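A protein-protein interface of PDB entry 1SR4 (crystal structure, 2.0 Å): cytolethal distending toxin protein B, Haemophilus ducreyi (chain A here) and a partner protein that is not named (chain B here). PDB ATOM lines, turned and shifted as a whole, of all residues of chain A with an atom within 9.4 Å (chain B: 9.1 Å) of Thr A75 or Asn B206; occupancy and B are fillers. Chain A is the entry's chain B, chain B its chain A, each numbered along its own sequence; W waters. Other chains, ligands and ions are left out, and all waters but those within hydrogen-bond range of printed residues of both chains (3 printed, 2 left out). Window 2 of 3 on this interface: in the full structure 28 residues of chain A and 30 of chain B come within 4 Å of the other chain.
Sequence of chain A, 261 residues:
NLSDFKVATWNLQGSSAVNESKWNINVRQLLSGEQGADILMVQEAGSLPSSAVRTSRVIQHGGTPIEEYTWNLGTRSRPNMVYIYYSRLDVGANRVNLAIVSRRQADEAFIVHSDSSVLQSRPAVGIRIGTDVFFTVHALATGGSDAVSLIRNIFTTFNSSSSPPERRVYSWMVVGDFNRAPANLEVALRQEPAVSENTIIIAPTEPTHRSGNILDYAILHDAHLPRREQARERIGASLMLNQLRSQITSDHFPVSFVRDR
Hydrophobic or aromatic side chains of chain B within 4 Å of the printed part of chain A: Leu B53 and Val B205.
Among the printed residues, no Asp or Glu carboxylate lies within 4 Å of a Lys or Arg side-chain nitrogen of the other chain.
The backbone carbonyl oxygen (O) of Gly A74 sits close to the backbone carbonyl oxygen (O) of Val B205, at 3.1 Å.
The backbone carbonyl oxygen (O) of Gln B51 is in hydrogen-bond range of the guanidinium group (NH2) of Arg A78 (2.8 Å).
Among the printed residues, merely in contact across the chains: Arg A28 with Val B205 (3.5 Å), Leu A73 with Val B205 (3.8 Å), Thr A75 with Leu B53 (3.6 Å), Thr A75 with Ala B204 (3.7 Å), Thr A75 with Val B205 (3.6 Å), Thr A75 with Asn B206 (3.8 Å) and Arg A78 with Leu B53 (3.5 Å).
Ser A51 touches none of the printed residues of chain B.
Printed residues of chain B within 4 Å of Leu A73: Val B205 (3.8 Å).
Gly A74 touches one residue of chain B.
Printed residues of chain B within 4 Å of Thr A75: Leu B53 (3.6 Å), Ala B204 (3.7 Å), Val B205 (3.6 Å) and Asn B206 (3.8 Å).
Of the printed residues of chain B, Arg A78 touches Gln B51 (2.8 Å) and Leu B53 (3.5 Å).
Leu B42 touches none of the printed residues of chain A.
Of chain A, only Thr A75 comes within 4 Å of Asn B206.
The nearest residue of chain B that does not touch Thr A75 is Thr B203 (6.1 Å).
The side-chain amide nitrogen of Asn A72 sits at hydrogen-bond distance from the backbone carbonyl oxygen of Thr A75.
The backbone NH (N) of Arg A78 lies within hydrogen-bond range of the side-chain hydroxyl (OG1) of Thr A75 (2.8 Å).
The backbone carbonyl oxygen of Asn A80 lies within hydrogen-bond range of the backbone NH of Leu A73 (2.8 Å).
OD1 of Asn A24 sits at hydrogen-bond distance from NH1 of Arg A28 (2.9 Å).
The guanidinium group of Arg A28 sits at hydrogen-bond distance from the backbone carbonyl oxygen of Leu A73, at 2.7 Å.
The side-chain hydroxyl of Thr A75 sits at hydrogen-bond distance from the side-chain hydroxyl of Ser A77, 3.4 Å away.
Water W1 bridges O of Ser A77 (2.7 Å) and N of Gln B51 (2.9 Å).
Water W3 lies within hydrogen-bond range of O of Leu B53 and NH1 of Arg A78.
Water W2 bridges O of Asn B206 and N of Arg A76.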
ATOM      1  N   ASN A  24      31.478 -32.114  13.235  1.00  0.00           N
ATOM      2  CA  ASN A  24      30.929 -30.997  12.476  1.00  0.00           C
ATOM      3  C   ASN A  24      31.052 -31.066  10.973  1.00  0.00           C
ATOM      4  O   ASN A  24      30.325 -30.373  10.266  1.00  0.00           O
ATOM      5  CB  ASN A  24      31.477 -29.687  13.016  1.00  0.00           C
ATOM      6  CG  ASN A  24      30.912 -29.374  14.383  1.00  0.00           C
ATOM      7  OD1 ASN A  24      29.695 -29.223  14.540  1.00  0.00           O
ATOM      8  ND2 ASN A  24      31.776 -29.311  15.385  1.00  0.00           N
ATOM      9  N   ARG A  28      27.490 -34.280  10.878  1.00  0.00           N
ATOM     10  CA  ARG A  28      26.427 -33.358  10.495  1.00  0.00           C
ATOM     11  C   ARG A  28      25.871 -33.705   9.113  1.00  0.00           C
ATOM     12  O   ARG A  28      24.668 -33.685   8.900  1.00  0.00           O
ATOM     13  CB  ARG A  28      26.931 -31.910  10.492  1.00  0.00           C
ATOM     14  CG  ARG A  28      27.451 -31.431  11.845  1.00  0.00           C
ATOM     15  CD  ARG A  28      27.945 -29.985  11.777  1.00  0.00           C
ATOM     16  NE  ARG A  28      26.820 -29.086  11.691  1.00  0.00           N
ATOM     17  CZ  ARG A  28      26.412 -28.305  12.676  1.00  0.00           C
ATOM     18  NH1 ARG A  28      27.049 -28.286  13.833  1.00  0.00           N
ATOM     19  NH2 ARG A  28      25.329 -27.585  12.506  1.00  0.00           N
ATOM     20  N   SER A  51      28.927 -28.198  21.659  1.00  0.00           N
ATOM     21  CA  SER A  51      27.631 -27.560  21.889  1.00  0.00           C
ATOM     22  C   SER A  51      26.539 -28.515  22.392  1.00  0.00           C
ATOM     23  O   SER A  51      25.416 -28.080  22.683  1.00  0.00           O
ATOM     24  CB  SER A  51      27.147 -26.852  20.622  1.00  0.00           C
ATOM     25  OG  SER A  51      26.749 -27.802  19.666  1.00  0.00           O
ATOM     26  N   TRP A  71      21.605 -31.975  20.855  1.00  0.00           N
ATOM     27  CA  TRP A  71      22.588 -31.261  20.063  1.00  0.00           C
ATOM     28  C   TRP A  71      21.833 -30.581  18.940  1.00  0.00           C
ATOM     29  O   TRP A  71      21.049 -31.221  18.247  1.00  0.00           O
ATOM     30  CB  TRP A  71      23.606 -32.265  19.519  1.00  0.00           C
ATOM     31  CG  TRP A  71      24.654 -31.688  18.624  1.00  0.00           C
ATOM     32  CD1 TRP A  71      25.273 -30.482  18.746  1.00  0.00           C
ATOM     33  CD2 TRP A  71      25.257 -32.339  17.500  1.00  0.00           C
ATOM     34  NE1 TRP A  71      26.229 -30.335  17.769  1.00  0.00           N
ATOM     35  CE2 TRP A  71      26.241 -31.464  16.990  1.00  0.00           C
ATOM     36  CE3 TRP A  71      25.064 -33.580  16.880  1.00  0.00           C
ATOM     37  CZ2 TRP A  71      27.032 -31.789  15.883  1.00  0.00           C
ATOM     38  CZ3 TRP A  71      25.852 -33.908  15.779  1.00  0.00           C
ATOM     39  CH2 TRP A  71      26.824 -33.011  15.292  1.00  0.00           C
ATOM     40  N   ASN A  72      22.061 -29.285  18.776  1.00  0.00           N
ATOM     41  CA  ASN A  72      21.366 -28.513  17.755  1.00  0.00           C
ATOM     42  C   ASN A  72      22.168 -28.422  16.466  1.00  0.00           C
ATOM     43  O   ASN A  72      23.198 -27.759  16.422  1.00  0.00           O
ATOM     44  CB  ASN A  72      21.064 -27.106  18.289  1.00  0.00           C
ATOM     45  CG  ASN A  72      20.244 -26.278  17.317  1.00  0.00           C
ATOM     46  OD1 ASN A  72      19.799 -26.784  16.275  1.00  0.00           O
ATOM     47  ND2 ASN A  72      20.037 -25.002  17.649  1.00  0.00           N
ATOM     48  N   LEU A  73      21.691 -29.086  15.417  1.00  0.00           N
ATOM     49  CA  LEU A  73      22.373 -29.079  14.120  1.00  0.00           C
ATOM     50  C   LEU A  73      22.051 -27.796  13.348  1.00  0.00           C
ATOM     51  O   LEU A  73      22.642 -27.521  12.299  1.00  0.00           O
ATOM     52  CB  LEU A  73      21.939 -30.295  13.286  1.00  0.00           C
ATOM     53  CG  LEU A  73      22.183 -31.684  13.887  1.00  0.00           C
ATOM     54  CD1 LEU A  73      21.449 -32.734  13.053  1.00  0.00           C
ATOM     55  CD2 LEU A  73      23.679 -31.981  13.932  1.00  0.00           C
ATOM     56  N   GLY A  74      21.089 -27.033  13.854  1.00  0.00           N
ATOM     57  CA  GLY A  74      20.732 -25.789  13.209  1.00  0.00           C
ATOM     58  C   GLY A  74      21.175 -24.602  14.047  1.00  0.00           C
ATOM     59  O   GLY A  74      22.049 -24.727  14.912  1.00  0.00           O
ATOM     60  N   THR A  75      20.571 -23.445  13.787  1.00  0.00           N
ATOM     61  CA  THR A  75      20.883 -22.213  14.504  1.00  0.00           C
ATOM     62  C   THR A  75      19.976 -22.065  15.738  1.00  0.00           C
ATOM     63  O   THR A  75      19.053 -22.851  15.935  1.00  0.00           O
ATOM     64  CB  THR A  75      20.656 -20.985  13.580  1.00  0.00           C
ATOM     65  OG1 THR A  75      19.269 -20.913  13.217  1.00  0.00           O
ATOM     66  CG2 THR A  75      21.489 -21.122  12.290  1.00  0.00           C
ATOM     67  N   ARG A  76      20.247 -21.069  16.579  1.00  0.00           N
ATOM     68  CA  ARG A  76      19.400 -20.849  17.743  1.00  0.00           C
ATOM     69  C   ARG A  76      17.998 -20.462  17.260  1.00  0.00           C
ATOM     70  O   ARG A  76      17.012 -20.904  17.837  1.00  0.00           O
ATOM     71  CB  ARG A  76      19.970 -19.733  18.639  1.00  0.00           C
ATOM     72  CG  ARG A  76      19.049 -19.358  19.828  1.00  0.00           C
ATOM     73  CD  ARG A  76      19.743 -18.401  20.814  1.00  0.00           C
ATOM     74  NE  ARG A  76      20.998 -18.978  21.292  1.00  0.00           N
ATOM     75  CZ  ARG A  76      21.091 -19.894  22.251  1.00  0.00           C
ATOM     76  NH1 ARG A  76      19.999 -20.339  22.857  1.00  0.00           N
ATOM     77  NH2 ARG A  76      22.278 -20.385  22.590  1.00  0.00           N
ATOM     78  N   SER A  77      17.901 -19.663  16.190  1.00  0.00           N
ATOM     79  CA  SER A  77      16.584 -19.263  15.707  1.00  0.00           C
ATOM     80  C   SER A  77      15.892 -20.347  14.886  1.00  0.00           C
ATOM     81  O   SER A  77      14.673 -20.366  14.796  1.00  0.00           O
ATOM     82  CB  SER A  77      16.664 -17.950  14.908  1.00  0.00           C
ATOM     83  OG  SER A  77      17.392 -18.118  13.720  1.00  0.00           O
ATOM     84  N   ARG A  78      16.654 -21.253  14.286  1.00  0.00           N
ATOM     85  CA  ARG A  78      16.045 -22.334  13.521  1.00  0.00           C
ATOM     86  C   ARG A  78      16.690 -23.646  13.932  1.00  0.00           C
ATOM     87  O   ARG A  78      17.511 -24.228  13.215  1.00  0.00           O
ATOM     88  CB  ARG A  78      16.168 -22.092  12.005  1.00  0.00           C
ATOM     89  CG  ARG A  78      15.160 -21.043  11.454  1.00  0.00           C
ATOM     90  CD  ARG A  78      13.691 -21.474  11.621  1.00  0.00           C
ATOM     91  NE  ARG A  78      13.498 -22.840  11.146  1.00  0.00           N
ATOM     92  CZ  ARG A  78      13.531 -23.207   9.870  1.00  0.00           C
ATOM     93  NH1 ARG A  78      13.368 -24.486   9.547  1.00  0.00           N
ATOM     94  NH2 ARG A  78      13.691 -22.293   8.911  1.00  0.00           N
ATOM     95  N   PRO A  79      16.329 -24.125  15.124  1.00  0.00           N
ATOM     96  CA  PRO A  79      16.875 -25.378  15.640  1.00  0.00           C
ATOM     97  C   PRO A  79      16.503 -26.607  14.813  1.00  0.00           C
ATOM     98  O   PRO A  79      15.470 -26.652  14.117  1.00  0.00           O
ATOM     99  CB  PRO A  79      16.342 -25.423  17.075  1.00  0.00           C
ATOM    100  CG  PRO A  79      15.070 -24.631  17.004  1.00  0.00           C
ATOM    101  CD  PRO A  79      15.414 -23.493  16.090  1.00  0.00           C
ATOM    102  N   ASN A  80      17.382 -27.595  14.883  1.00  0.00           N
ATOM    103  CA  ASN A  80      17.226 -28.852  14.173  1.00  0.00           C
ATOM    104  C   ASN A  80      17.889 -29.812  15.153  1.00  0.00           C
ATOM    105  O   ASN A  80      19.075 -30.136  15.034  1.00  0.00           O
ATOM    106  CB  ASN A  80      17.976 -28.771  12.839  1.00  0.00           C
ATOM    107  CG  ASN A  80      17.952 -30.073  12.074  1.00  0.00           C
ATOM    108  OD1 ASN A  80      17.182 -30.984  12.376  1.00  0.00           O
ATOM    109  ND2 ASN A  80      18.791 -30.160  11.059  1.00  0.00           N
ATOM    110  N   MET A  81      17.096 -30.259  16.120  1.00  0.00           N
ATOM    111  CA  MET A  81      17.572 -31.092  17.216  1.00  0.00           C
ATOM    112  C   MET A  81      17.642 -32.587  17.070  1.00  0.00           C
ATOM    113  O   MET A  81      16.780 -33.203  16.461  1.00  0.00           O
ATOM    114  CB  MET A  81      16.717 -30.837  18.462  1.00  0.00           C
ATOM    115  CG  MET A  81      16.429 -29.391  18.800  1.00  0.00           C
ATOM    116  SD  MET A  81      17.917 -28.510  19.236  1.00  0.00           S
ATOM    117  CE  MET A  81      18.654 -29.627  20.459  1.00  0.00           C
ATOM    118  N   LEU B  42      11.971 -12.201  15.225  1.00  0.00           N
ATOM    119  CA  LEU B  42      12.129 -13.576  15.701  1.00  0.00           C
ATOM    120  C   LEU B  42      10.977 -13.912  16.658  1.00  0.00           C
ATOM    121  O   LEU B  42      10.666 -15.083  16.885  1.00  0.00           O
ATOM    122  CB  LEU B  42      13.495 -13.775  16.380  1.00  0.00           C
ATOM    123  CG  LEU B  42      14.656 -14.118  15.424  1.00  0.00           C
ATOM    124  CD1 LEU B  42      14.757 -13.047  14.345  1.00  0.00           C
ATOM    125  CD2 LEU B  42      15.971 -14.211  16.184  1.00  0.00           C
ATOM    126  N   GLN B  51      12.103 -18.083  11.020  1.00  0.00           N
ATOM    127  CA  GLN B  51      12.954 -17.368  10.086  1.00  0.00           C
ATOM    128  C   GLN B  51      13.292 -18.309   8.942  1.00  0.00           C
ATOM    129  O   GLN B  51      13.180 -19.527   9.063  1.00  0.00           O
ATOM    130  CB  GLN B  51      14.241 -16.890  10.767  1.00  0.00           C
ATOM    131  CG  GLN B  51      13.977 -15.931  11.919  1.00  0.00           C
ATOM    132  CD  GLN B  51      13.256 -14.676  11.457  1.00  0.00           C
ATOM    133  OE1 GLN B  51      13.853 -13.805  10.828  1.00  0.00           O
ATOM    134  NE2 GLN B  51      11.959 -14.589  11.749  1.00  0.00           N
ATOM    135  N   VAL B  52      13.683 -17.725   7.822  1.00  0.00           N
ATOM    136  CA  VAL B  52      14.056 -18.492   6.647  1.00  0.00           C
ATOM    137  C   VAL B  52      15.451 -19.119   6.807  1.00  0.00           C
ATOM    138  O   VAL B  52      16.403 -18.421   7.132  1.00  0.00           O
ATOM    139  CB  VAL B  52      14.086 -17.577   5.394  1.00  0.00           C
ATOM    140  CG1 VAL B  52      14.558 -18.369   4.164  1.00  0.00           C
ATOM    141  CG2 VAL B  52      12.707 -16.986   5.149  1.00  0.00           C
ATOM    142  N   LEU B  53      15.553 -20.433   6.602  1.00  0.00           N
ATOM    143  CA  LEU B  53      16.836 -21.166   6.626  1.00  0.00           C
ATOM    144  C   LEU B  53      16.528 -22.445   5.849  1.00  0.00           C
ATOM    145  O   LEU B  53      16.195 -23.470   6.430  1.00  0.00           O
ATOM    146  CB  LEU B  53      17.311 -21.499   8.049  1.00  0.00           C
ATOM    147  CG  LEU B  53      18.849 -21.595   8.153  1.00  0.00           C
ATOM    148  CD1 LEU B  53      19.284 -21.970   9.555  1.00  0.00           C
ATOM    149  CD2 LEU B  53      19.367 -22.650   7.170  1.00  0.00           C
ATOM    150  N   THR B 203      23.867 -21.162   3.655  1.00  0.00           N
ATOM    151  CA  THR B 203      23.433 -20.460   4.850  1.00  0.00           C
ATOM    152  C   THR B 203      24.166 -21.098   6.028  1.00  0.00           C
ATOM    153  O   THR B 203      24.121 -22.317   6.196  1.00  0.00           O
ATOM    154  CB  THR B 203      21.887 -20.588   5.045  1.00  0.00           C
ATOM    155  OG1 THR B 203      21.209 -20.053   3.897  1.00  0.00           O
ATOM    156  CG2 THR B 203      21.430 -19.828   6.294  1.00  0.00           C
ATOM    157  N   ALA B 204      24.863 -20.284   6.823  1.00  0.00           N
ATOM    158  CA  ALA B 204      25.588 -20.788   7.997  1.00  0.00           C
ATOM    159  C   ALA B 204      24.602 -21.320   9.036  1.00  0.00           C
ATOM    160  O   ALA B 204      23.569 -20.695   9.307  1.00  0.00           O
ATOM    161  CB  ALA B 204      26.445 -19.676   8.617  1.00  0.00           C
ATOM    162  N   VAL B 205      24.929 -22.463   9.627  1.00  0.00           N
ATOM    163  CA  VAL B 205      24.056 -23.088  10.604  1.00  0.00           C
ATOM    164  C   VAL B 205      24.696 -23.224  11.977  1.00  0.00           C
ATOM    165  O   VAL B 205      24.211 -23.979  12.812  1.00  0.00           O
ATOM    166  CB  VAL B 205      23.594 -24.487  10.131  1.00  0.00           C
ATOM    167  CG1 VAL B 205      22.742 -24.358   8.900  1.00  0.00           C
ATOM    168  CG2 VAL B 205      24.804 -25.380   9.852  1.00  0.00           C
ATOM    169  N   ASN B 206      25.776 -22.477  12.202  1.00  0.00           N
ATOM    170  CA  ASN B 206      26.484 -22.486  13.481  1.00  0.00           C
ATOM    171  C   ASN B 206      25.609 -21.899  14.587  1.00  0.00           C
ATOM    172  O   ASN B 206      24.724 -21.086  14.265  1.00  0.00           O
ATOM    173  CB  ASN B 206      27.786 -21.669  13.376  1.00  0.00           C
ATOM    174  CG  ASN B 206      27.566 -20.239  12.841  1.00  0.00           C
ATOM    175  OD1 ASN B 206      26.902 -20.029  11.824  1.00  0.00           O
ATOM    176  ND2 ASN B 206      28.157 -19.258  13.523  1.00  0.00           N
ATOM    177  OXT ASN B 206      25.831 -22.244  15.764  1.00  0.00           O
HETATM  178  O   HOH W   1      13.075 -18.493  13.760  1.00  0.00           O
HETATM  179  O   HOH W   2      23.198 -20.140  16.404  1.00  0.00           O
HETATM  180  O   HOH W   3      14.206 -25.224   6.989  1.00  0.00           O
